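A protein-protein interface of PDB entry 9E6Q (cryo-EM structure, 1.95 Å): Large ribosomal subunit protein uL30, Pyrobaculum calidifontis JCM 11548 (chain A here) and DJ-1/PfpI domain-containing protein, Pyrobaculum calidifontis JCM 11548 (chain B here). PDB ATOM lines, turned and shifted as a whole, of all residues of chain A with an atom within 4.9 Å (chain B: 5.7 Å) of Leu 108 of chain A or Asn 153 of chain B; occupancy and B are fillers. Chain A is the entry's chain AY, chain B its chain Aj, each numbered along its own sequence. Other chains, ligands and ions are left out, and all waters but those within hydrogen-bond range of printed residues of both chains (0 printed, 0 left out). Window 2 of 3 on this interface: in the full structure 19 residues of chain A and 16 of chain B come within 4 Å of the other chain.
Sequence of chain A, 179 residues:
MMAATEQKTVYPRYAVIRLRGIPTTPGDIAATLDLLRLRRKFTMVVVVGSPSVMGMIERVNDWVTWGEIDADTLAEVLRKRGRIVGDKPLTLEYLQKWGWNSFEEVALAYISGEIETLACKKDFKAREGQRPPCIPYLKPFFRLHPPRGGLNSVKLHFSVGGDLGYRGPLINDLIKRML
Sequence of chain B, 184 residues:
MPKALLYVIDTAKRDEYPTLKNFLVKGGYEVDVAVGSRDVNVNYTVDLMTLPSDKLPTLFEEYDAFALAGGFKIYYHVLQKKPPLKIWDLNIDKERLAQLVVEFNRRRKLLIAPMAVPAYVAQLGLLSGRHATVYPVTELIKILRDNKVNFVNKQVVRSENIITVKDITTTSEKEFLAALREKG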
ATOM      1  N   ALA A  71      25.106 -14.722  -9.282  1.00  0.00           N
ATOM      2  CA  ALA A  71      25.386 -14.038 -10.539  1.00  0.00           C
ATOM      3  C   ALA A  71      24.161 -13.306 -11.073  1.00  0.00           C
ATOM      4  O   ALA A  71      24.285 -12.221 -11.648  1.00  0.00           O
ATOM      5  CB  ALA A  71      25.908 -15.035 -11.568  1.00  0.00           C
ATOM      6  N   ASP A  72      22.973 -13.887 -10.918  1.00  0.00           N
ATOM      7  CA  ASP A  72      21.778 -13.234 -11.441  1.00  0.00           C
ATOM      8  C   ASP A  72      21.454 -11.966 -10.667  1.00  0.00           C
ATOM      9  O   ASP A  72      21.035 -10.964 -11.255  1.00  0.00           O
ATOM     10  CB  ASP A  72      20.594 -14.190 -11.417  1.00  0.00           C
ATOM     11  CG  ASP A  72      20.543 -15.066 -12.639  1.00  0.00           C
ATOM     12  OD1 ASP A  72      20.775 -16.280 -12.496  1.00  0.00           O
ATOM     13  OD2 ASP A  72      20.293 -14.544 -13.747  1.00  0.00           O
ATOM     14  N   GLU A 104      24.670 -10.358 -17.914  1.00  0.00           N
ATOM     15  CA  GLU A 104      24.752 -11.694 -17.336  1.00  0.00           C
ATOM     16  C   GLU A 104      26.140 -12.291 -17.506  1.00  0.00           C
ATOM     17  O   GLU A 104      26.660 -12.935 -16.590  1.00  0.00           O
ATOM     18  CB  GLU A 104      23.703 -12.600 -17.975  1.00  0.00           C
ATOM     19  CG  GLU A 104      22.320 -12.471 -17.368  1.00  0.00           C
ATOM     20  CD  GLU A 104      21.599 -11.219 -17.825  1.00  0.00           C
ATOM     21  OE1 GLU A 104      22.115 -10.527 -18.726  1.00  0.00           O
ATOM     22  OE2 GLU A 104      20.518 -10.920 -17.277  1.00  0.00           O
ATOM     23  N   GLU A 105      26.756 -12.093 -18.673  1.00  0.00           N
ATOM     24  CA  GLU A 105      28.054 -12.707 -18.925  1.00  0.00           C
ATOM     25  C   GLU A 105      29.139 -12.122 -18.027  1.00  0.00           C
ATOM     26  O   GLU A 105      29.966 -12.861 -17.486  1.00  0.00           O
ATOM     27  CB  GLU A 105      28.427 -12.563 -20.398  1.00  0.00           C
ATOM     28  CG  GLU A 105      29.910 -12.685 -20.659  1.00  0.00           C
ATOM     29  CD  GLU A 105      30.291 -12.318 -22.071  1.00  0.00           C
ATOM     30  OE1 GLU A 105      31.500 -12.246 -22.365  1.00  0.00           O
ATOM     31  OE2 GLU A 105      29.381 -12.118 -22.893  1.00  0.00           O
ATOM     32  N   VAL A 106      29.158 -10.800 -17.856  1.00  0.00           N
ATOM     33  CA  VAL A 106      30.196 -10.198 -17.026  1.00  0.00           C
ATOM     34  C   VAL A 106      29.979 -10.545 -15.557  1.00  0.00           C
ATOM     35  O   VAL A 106      30.939 -10.783 -14.817  1.00  0.00           O
ATOM     36  CB  VAL A 106      30.278  -8.678 -17.262  1.00  0.00           C
ATOM     37  CG1 VAL A 106      29.072  -7.963 -16.711  1.00  0.00           C
ATOM     38  CG2 VAL A 106      31.550  -8.120 -16.657  1.00  0.00           C
ATOM     39  N   ALA A 107      28.722 -10.597 -15.114  1.00  0.00           N
ATOM     40  CA  ALA A 107      28.445 -10.974 -13.736  1.00  0.00           C
ATOM     41  C   ALA A 107      28.874 -12.406 -13.471  1.00  0.00           C
ATOM     42  O   ALA A 107      29.463 -12.707 -12.430  1.00  0.00           O
ATOM     43  CB  ALA A 107      26.961 -10.786 -13.427  1.00  0.00           C
ATOM     44  N   LEU A 108      28.584 -13.307 -14.407  1.00  0.00           N
ATOM     45  CA  LEU A 108      29.010 -14.690 -14.249  1.00  0.00           C
ATOM     46  C   LEU A 108      30.527 -14.803 -14.278  1.00  0.00           C
ATOM     47  O   LEU A 108      31.111 -15.578 -13.516  1.00  0.00           O
ATOM     48  CB  LEU A 108      28.388 -15.560 -15.334  1.00  0.00           C
ATOM     49  CG  LEU A 108      28.813 -17.020 -15.268  1.00  0.00           C
ATOM     50  CD1 LEU A 108      28.312 -17.645 -13.980  1.00  0.00           C
ATOM     51  CD2 LEU A 108      28.314 -17.781 -16.478  1.00  0.00           C
ATOM     52  N   ALA A 109      31.182 -14.037 -15.150  1.00  0.00           N
ATOM     53  CA  ALA A 109      32.639 -14.057 -15.202  1.00  0.00           C
ATOM     54  C   ALA A 109      33.243 -13.660 -13.863  1.00  0.00           C
ATOM     55  O   ALA A 109      34.286 -14.181 -13.467  1.00  0.00           O
ATOM     56  CB  ALA A 109      33.137 -13.130 -16.306  1.00  0.00           C
ATOM     57  N   TYR A 110      32.600 -12.738 -13.152  1.00  0.00           N
ATOM     58  CA  TYR A 110      33.140 -12.280 -11.882  1.00  0.00           C
ATOM     59  C   TYR A 110      32.808 -13.242 -10.751  1.00  0.00           C
ATOM     60  O   TYR A 110      33.667 -13.557  -9.926  1.00  0.00           O
ATOM     61  CB  TYR A 110      32.616 -10.885 -11.569  1.00  0.00           C
ATOM     62  CG  TYR A 110      33.068 -10.365 -10.239  1.00  0.00           C
ATOM     63  CD1 TYR A 110      34.404 -10.126  -9.985  1.00  0.00           C
ATOM     64  CD2 TYR A 110      32.158 -10.117  -9.234  1.00  0.00           C
ATOM     65  CE1 TYR A 110      34.820  -9.653  -8.772  1.00  0.00           C
ATOM     66  CE2 TYR A 110      32.563  -9.647  -8.024  1.00  0.00           C
ATOM     67  CZ  TYR A 110      33.894  -9.415  -7.792  1.00  0.00           C
ATOM     68  OH  TYR A 110      34.291  -8.940  -6.572  1.00  0.00           O
ATOM     69  N   ILE A 111      31.563 -13.708 -10.692  1.00  0.00           N
ATOM     70  CA  ILE A 111      31.171 -14.625  -9.630  1.00  0.00           C
ATOM     71  C   ILE A 111      31.930 -15.936  -9.758  1.00  0.00           C
ATOM     72  O   ILE A 111      32.409 -16.490  -8.763  1.00  0.00           O
ATOM     73  CB  ILE A 111      29.649 -14.843  -9.644  1.00  0.00           C
ATOM     74  CG1 ILE A 111      28.927 -13.523  -9.376  1.00  0.00           C
ATOM     75  CG2 ILE A 111      29.246 -15.869  -8.619  1.00  0.00           C
ATOM     76  CD1 ILE A 111      29.298 -12.877  -8.076  1.00  0.00           C
ATOM     77  N   SER A 112      32.065 -16.447 -10.981  1.00  0.00           N
ATOM     78  CA  SER A 112      32.714 -17.737 -11.172  1.00  0.00           C
ATOM     79  C   SER A 112      34.222 -17.671 -10.981  1.00  0.00           C
ATOM     80  O   SER A 112      34.850 -18.711 -10.775  1.00  0.00           O
ATOM     81  CB  SER A 112      32.394 -18.291 -12.555  1.00  0.00           C
ATOM     82  OG  SER A 112      32.983 -17.491 -13.558  1.00  0.00           O
ATOM     83  N   GLY A 113      34.816 -16.488 -11.036  1.00  0.00           N
ATOM     84  CA  GLY A 113      36.243 -16.350 -10.865  1.00  0.00           C
ATOM     85  C   GLY A 113      37.043 -16.190 -12.135  1.00  0.00           C
ATOM     86  O   GLY A 113      38.274 -16.153 -12.064  1.00  0.00           O
ATOM     87  N   THR B 133      22.228 -26.659 -14.049  1.00  0.00           N
ATOM     88  CA  THR B 133      22.370 -25.326 -13.498  1.00  0.00           C
ATOM     89  C   THR B 133      22.287 -25.414 -11.982  1.00  0.00           C
ATOM     90  O   THR B 133      21.868 -26.428 -11.425  1.00  0.00           O
ATOM     91  CB  THR B 133      21.301 -24.375 -14.049  1.00  0.00           C
ATOM     92  OG1 THR B 133      21.732 -23.024 -13.873  1.00  0.00           O
ATOM     93  CG2 THR B 133      19.983 -24.573 -13.339  1.00  0.00           C
ATOM     94  N   PRO B 136      23.683 -19.626  -8.697  1.00  0.00           N
ATOM     95  CA  PRO B 136      24.997 -19.239  -9.228  1.00  0.00           C
ATOM     96  C   PRO B 136      25.826 -18.424  -8.242  1.00  0.00           C
ATOM     97  O   PRO B 136      26.142 -17.259  -8.469  1.00  0.00           O
ATOM     98  CB  PRO B 136      24.622 -18.436 -10.480  1.00  0.00           C
ATOM     99  CG  PRO B 136      23.203 -18.035 -10.311  1.00  0.00           C
ATOM    100  CD  PRO B 136      22.630 -18.685  -9.095  1.00  0.00           C
ATOM    101  N   ILE B 141      28.960 -23.159  -7.912  1.00  0.00           N
ATOM    102  CA  ILE B 141      29.428 -23.377  -9.276  1.00  0.00           C
ATOM    103  C   ILE B 141      30.684 -24.232  -9.267  1.00  0.00           C
ATOM    104  O   ILE B 141      30.863 -25.108 -10.118  1.00  0.00           O
ATOM    105  CB  ILE B 141      29.666 -22.030  -9.982  1.00  0.00           C
ATOM    106  CG1 ILE B 141      28.348 -21.288 -10.186  1.00  0.00           C
ATOM    107  CG2 ILE B 141      30.347 -22.240 -11.313  1.00  0.00           C
ATOM    108  CD1 ILE B 141      28.525 -19.846 -10.545  1.00  0.00           C
ATOM    109  N   ARG B 145      31.527 -28.031 -11.000  1.00  0.00           N
ATOM    110  CA  ARG B 145      32.660 -28.267 -11.886  1.00  0.00           C
ATOM    111  C   ARG B 145      33.611 -29.313 -11.323  1.00  0.00           C
ATOM    112  O   ARG B 145      34.222 -30.063 -12.090  1.00  0.00           O
ATOM    113  CB  ARG B 145      33.392 -26.956 -12.144  1.00  0.00           C
ATOM    114  CG  ARG B 145      32.495 -25.869 -12.705  1.00  0.00           C
ATOM    115  CD  ARG B 145      33.188 -25.084 -13.788  1.00  0.00           C
ATOM    116  NE  ARG B 145      32.274 -24.216 -14.515  1.00  0.00           N
ATOM    117  CZ  ARG B 145      32.470 -22.920 -14.710  1.00  0.00           C
ATOM    118  NH1 ARG B 145      33.505 -22.290 -14.181  1.00  0.00           N
ATOM    119  NH2 ARG B 145      31.611 -22.240 -15.460  1.00  0.00           N
ATOM    120  N   PHE B 151      28.280 -26.683 -16.140  1.00  0.00           N
ATOM    121  CA  PHE B 151      27.397 -25.633 -15.661  1.00  0.00           C
ATOM    122  C   PHE B 151      26.825 -24.860 -16.838  1.00  0.00           C
ATOM    123  O   PHE B 151      27.560 -24.449 -17.739  1.00  0.00           O
ATOM    124  CB  PHE B 151      28.138 -24.684 -14.723  1.00  0.00           C
ATOM    125  CG  PHE B 151      27.305 -23.528 -14.263  1.00  0.00           C
ATOM    126  CD1 PHE B 151      26.239 -23.726 -13.409  1.00  0.00           C
ATOM    127  CD2 PHE B 151      27.573 -22.247 -14.700  1.00  0.00           C
ATOM    128  CE1 PHE B 151      25.466 -22.674 -12.995  1.00  0.00           C
ATOM    129  CE2 PHE B 151      26.801 -21.189 -14.284  1.00  0.00           C
ATOM    130  CZ  PHE B 151      25.747 -21.402 -13.432  1.00  0.00           C
ATOM    131  N   VAL B 152      25.514 -24.664 -16.828  1.00  0.00           N
ATOM    132  CA  VAL B 152      24.822 -23.864 -17.827  1.00  0.00           C
ATOM    133  C   VAL B 152      24.140 -22.708 -17.113  1.00  0.00           C
ATOM    134  O   VAL B 152      23.578 -22.881 -16.028  1.00  0.00           O
ATOM    135  CB  VAL B 152      23.802 -24.701 -18.623  1.00  0.00           C
ATOM    136  CG1 VAL B 152      23.108 -23.849 -19.662  1.00  0.00           C
ATOM    137  CG2 VAL B 152      24.488 -25.871 -19.282  1.00  0.00           C
ATOM    138  N   ASN B 153      24.178 -21.532 -17.730  1.00  0.00           N
ATOM    139  CA  ASN B 153      23.680 -20.302 -17.125  1.00  0.00           C
ATOM    140  C   ASN B 153      22.242 -20.008 -17.525  1.00  0.00           C
ATOM    141  O   ASN B 153      21.867 -18.854 -17.722  1.00  0.00           O
ATOM    142  CB  ASN B 153      24.592 -19.137 -17.485  1.00  0.00           C
ATOM    143  CG  ASN B 153      24.496 -17.995 -16.501  1.00  0.00           C
ATOM    144  OD1 ASN B 153      23.979 -18.151 -15.398  1.00  0.00           O
ATOM    145  ND2 ASN B 153      24.999 -16.834 -16.896  1.00  0.00           N
ATOM    146  N   LYS B 154      21.422 -21.042 -17.672  1.00  0.00           N
ATOM    147  CA  LYS B 154      19.997 -20.892 -17.917  1.00  0.00           C
ATOM    148  C   LYS B 154      19.222 -21.096 -16.622  1.00  0.00           C
ATOM    149  O   LYS B 154      19.699 -21.745 -15.691  1.00  0.00           O
ATOM    150  CB  LYS B 154      19.519 -21.882 -18.977  1.00  0.00           C
ATOM    151  CG  LYS B 154      19.422 -21.282 -20.365  1.00  0.00           C
ATOM    152  CD  LYS B 154      19.161 -22.337 -21.426  1.00  0.00           C
ATOM    153  CE  LYS B 154      18.123 -23.352 -20.973  1.00  0.00           C
ATOM    154  NZ  LYS B 154      16.762 -22.758 -20.868  1.00  0.00           N
ATOM    155  N   GLN B 155      18.019 -20.524 -16.567  1.00  0.00           N
ATOM    156  CA  GLN B 155      17.224 -20.591 -15.344  1.00  0.00           C
ATOM    157  C   GLN B 155      16.811 -22.022 -15.025  1.00  0.00           C
ATOM    158  O   GLN B 155      16.920 -22.469 -13.880  1.00  0.00           O
ATOM    159  CB  GLN B 155      15.995 -19.692 -15.466  1.00  0.00           C
ATOM    160  CG  GLN B 155      15.060 -19.757 -14.274  1.00  0.00           C
ATOM    161  CD  GLN B 155      15.605 -19.047 -13.051  1.00  0.00           C
ATOM    162  OE1 GLN B 155      16.467 -18.182 -13.155  1.00  0.00           O
ATOM    163  NE2 GLN B 155      15.103 -19.415 -11.882  1.00  0.00           N
ATOM    164  N   LYS B 166      17.772 -22.749 -11.043  1.00  0.00           N
ATOM    165  CA  LYS B 166      18.631 -21.878 -10.248  1.00  0.00           C
ATOM    166  C   LYS B 166      17.957 -21.473  -8.946  1.00  0.00           C
ATOM    167  O   LYS B 166      18.566 -21.529  -7.874  1.00  0.00           O
ATOM    168  CB  LYS B 166      19.016 -20.647 -11.054  1.00  0.00           C
ATOM    169  CG  LYS B 166      20.115 -20.892 -12.043  1.00  0.00           C
ATOM    170  CD  LYS B 166      20.799 -19.600 -12.391  1.00  0.00           C
ATOM    171  CE  LYS B 166      20.299 -19.036 -13.687  1.00  0.00           C
ATOM    172  NZ  LYS B 166      21.436 -18.650 -14.551  1.00  0.00           N
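The backbone NH (N) of Lys 166 of chain B is in hydrogen-bond range of the backbone carbonyl oxygen (O) of Gln 155 of chain B, at 3.0 Å. O of Leu 108 of chain A is in hydrogen-bond range of OG of Ser 112 of chain A (2.7 Å). The side-chain amino group of Lys 166 of chain B lies within hydrogen-bond range of the side-chain amide oxygen of Asn 153 of chain B (2.7 Å).
Leu 108 of chain A touches just these residues of chain B: Phe 151 and Asn 153. Asn 153 of chain B touches just one residue of chain A: Leu 108. Of the printed residues of chain B, Ala 71 of chain A touches Pro 136. Printed residues of chain A within 4 Å of Lys 166 of chain B: Asp 72. The nearest residue of chain B that does not touch Leu 108 of chain A is Ile 141 of chain B (4.1 Å). The nearest residue of chain A that does not touch Asn 153 of chain B is Glu 104 of chain A (4.2 Å). The nearest printed residue of chain A that does not touch Lys 166 of chain B is Ala 71 of chain A (6.5 Å).
OD1 of Asp 72 of chain A touches CG of Pro 136 of chain B, 3.7 Å away. Phe 151 of chain B touches Leu 108 of chain A (CE2 to CD1, 3.9 Å). ND2 of Asn 153 of chain B touches CD2 of Leu 108 of chain A, 3.5 Å away. Pro 136 of chain B touches Ile 111 of chain A (O to CG2, 3.4 Å).
Of the 12 printed residues of chain A, 4 touch a printed residue of chain B. Hydrophobic or aromatic side chains of chain A that line the printed part of chain B: Ala 71, Leu 108 and Ile 111. Hydrophobic or aromatic side chains of chain B within 4 Å of the printed part of chain A: Pro 136 and Phe 151. Among the printed residues, 6 pairs touch across the chains.
OD1 of Asp 72 of chain A lies within salt-bridge range of NZ of Lys 166 of chain B, at 3.2 Å. The backbone carbonyl oxygen (O) of Pro 136 of chain B is in hydrogen-bond range of the backbone NH (N) of Ala 71 of chain A.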
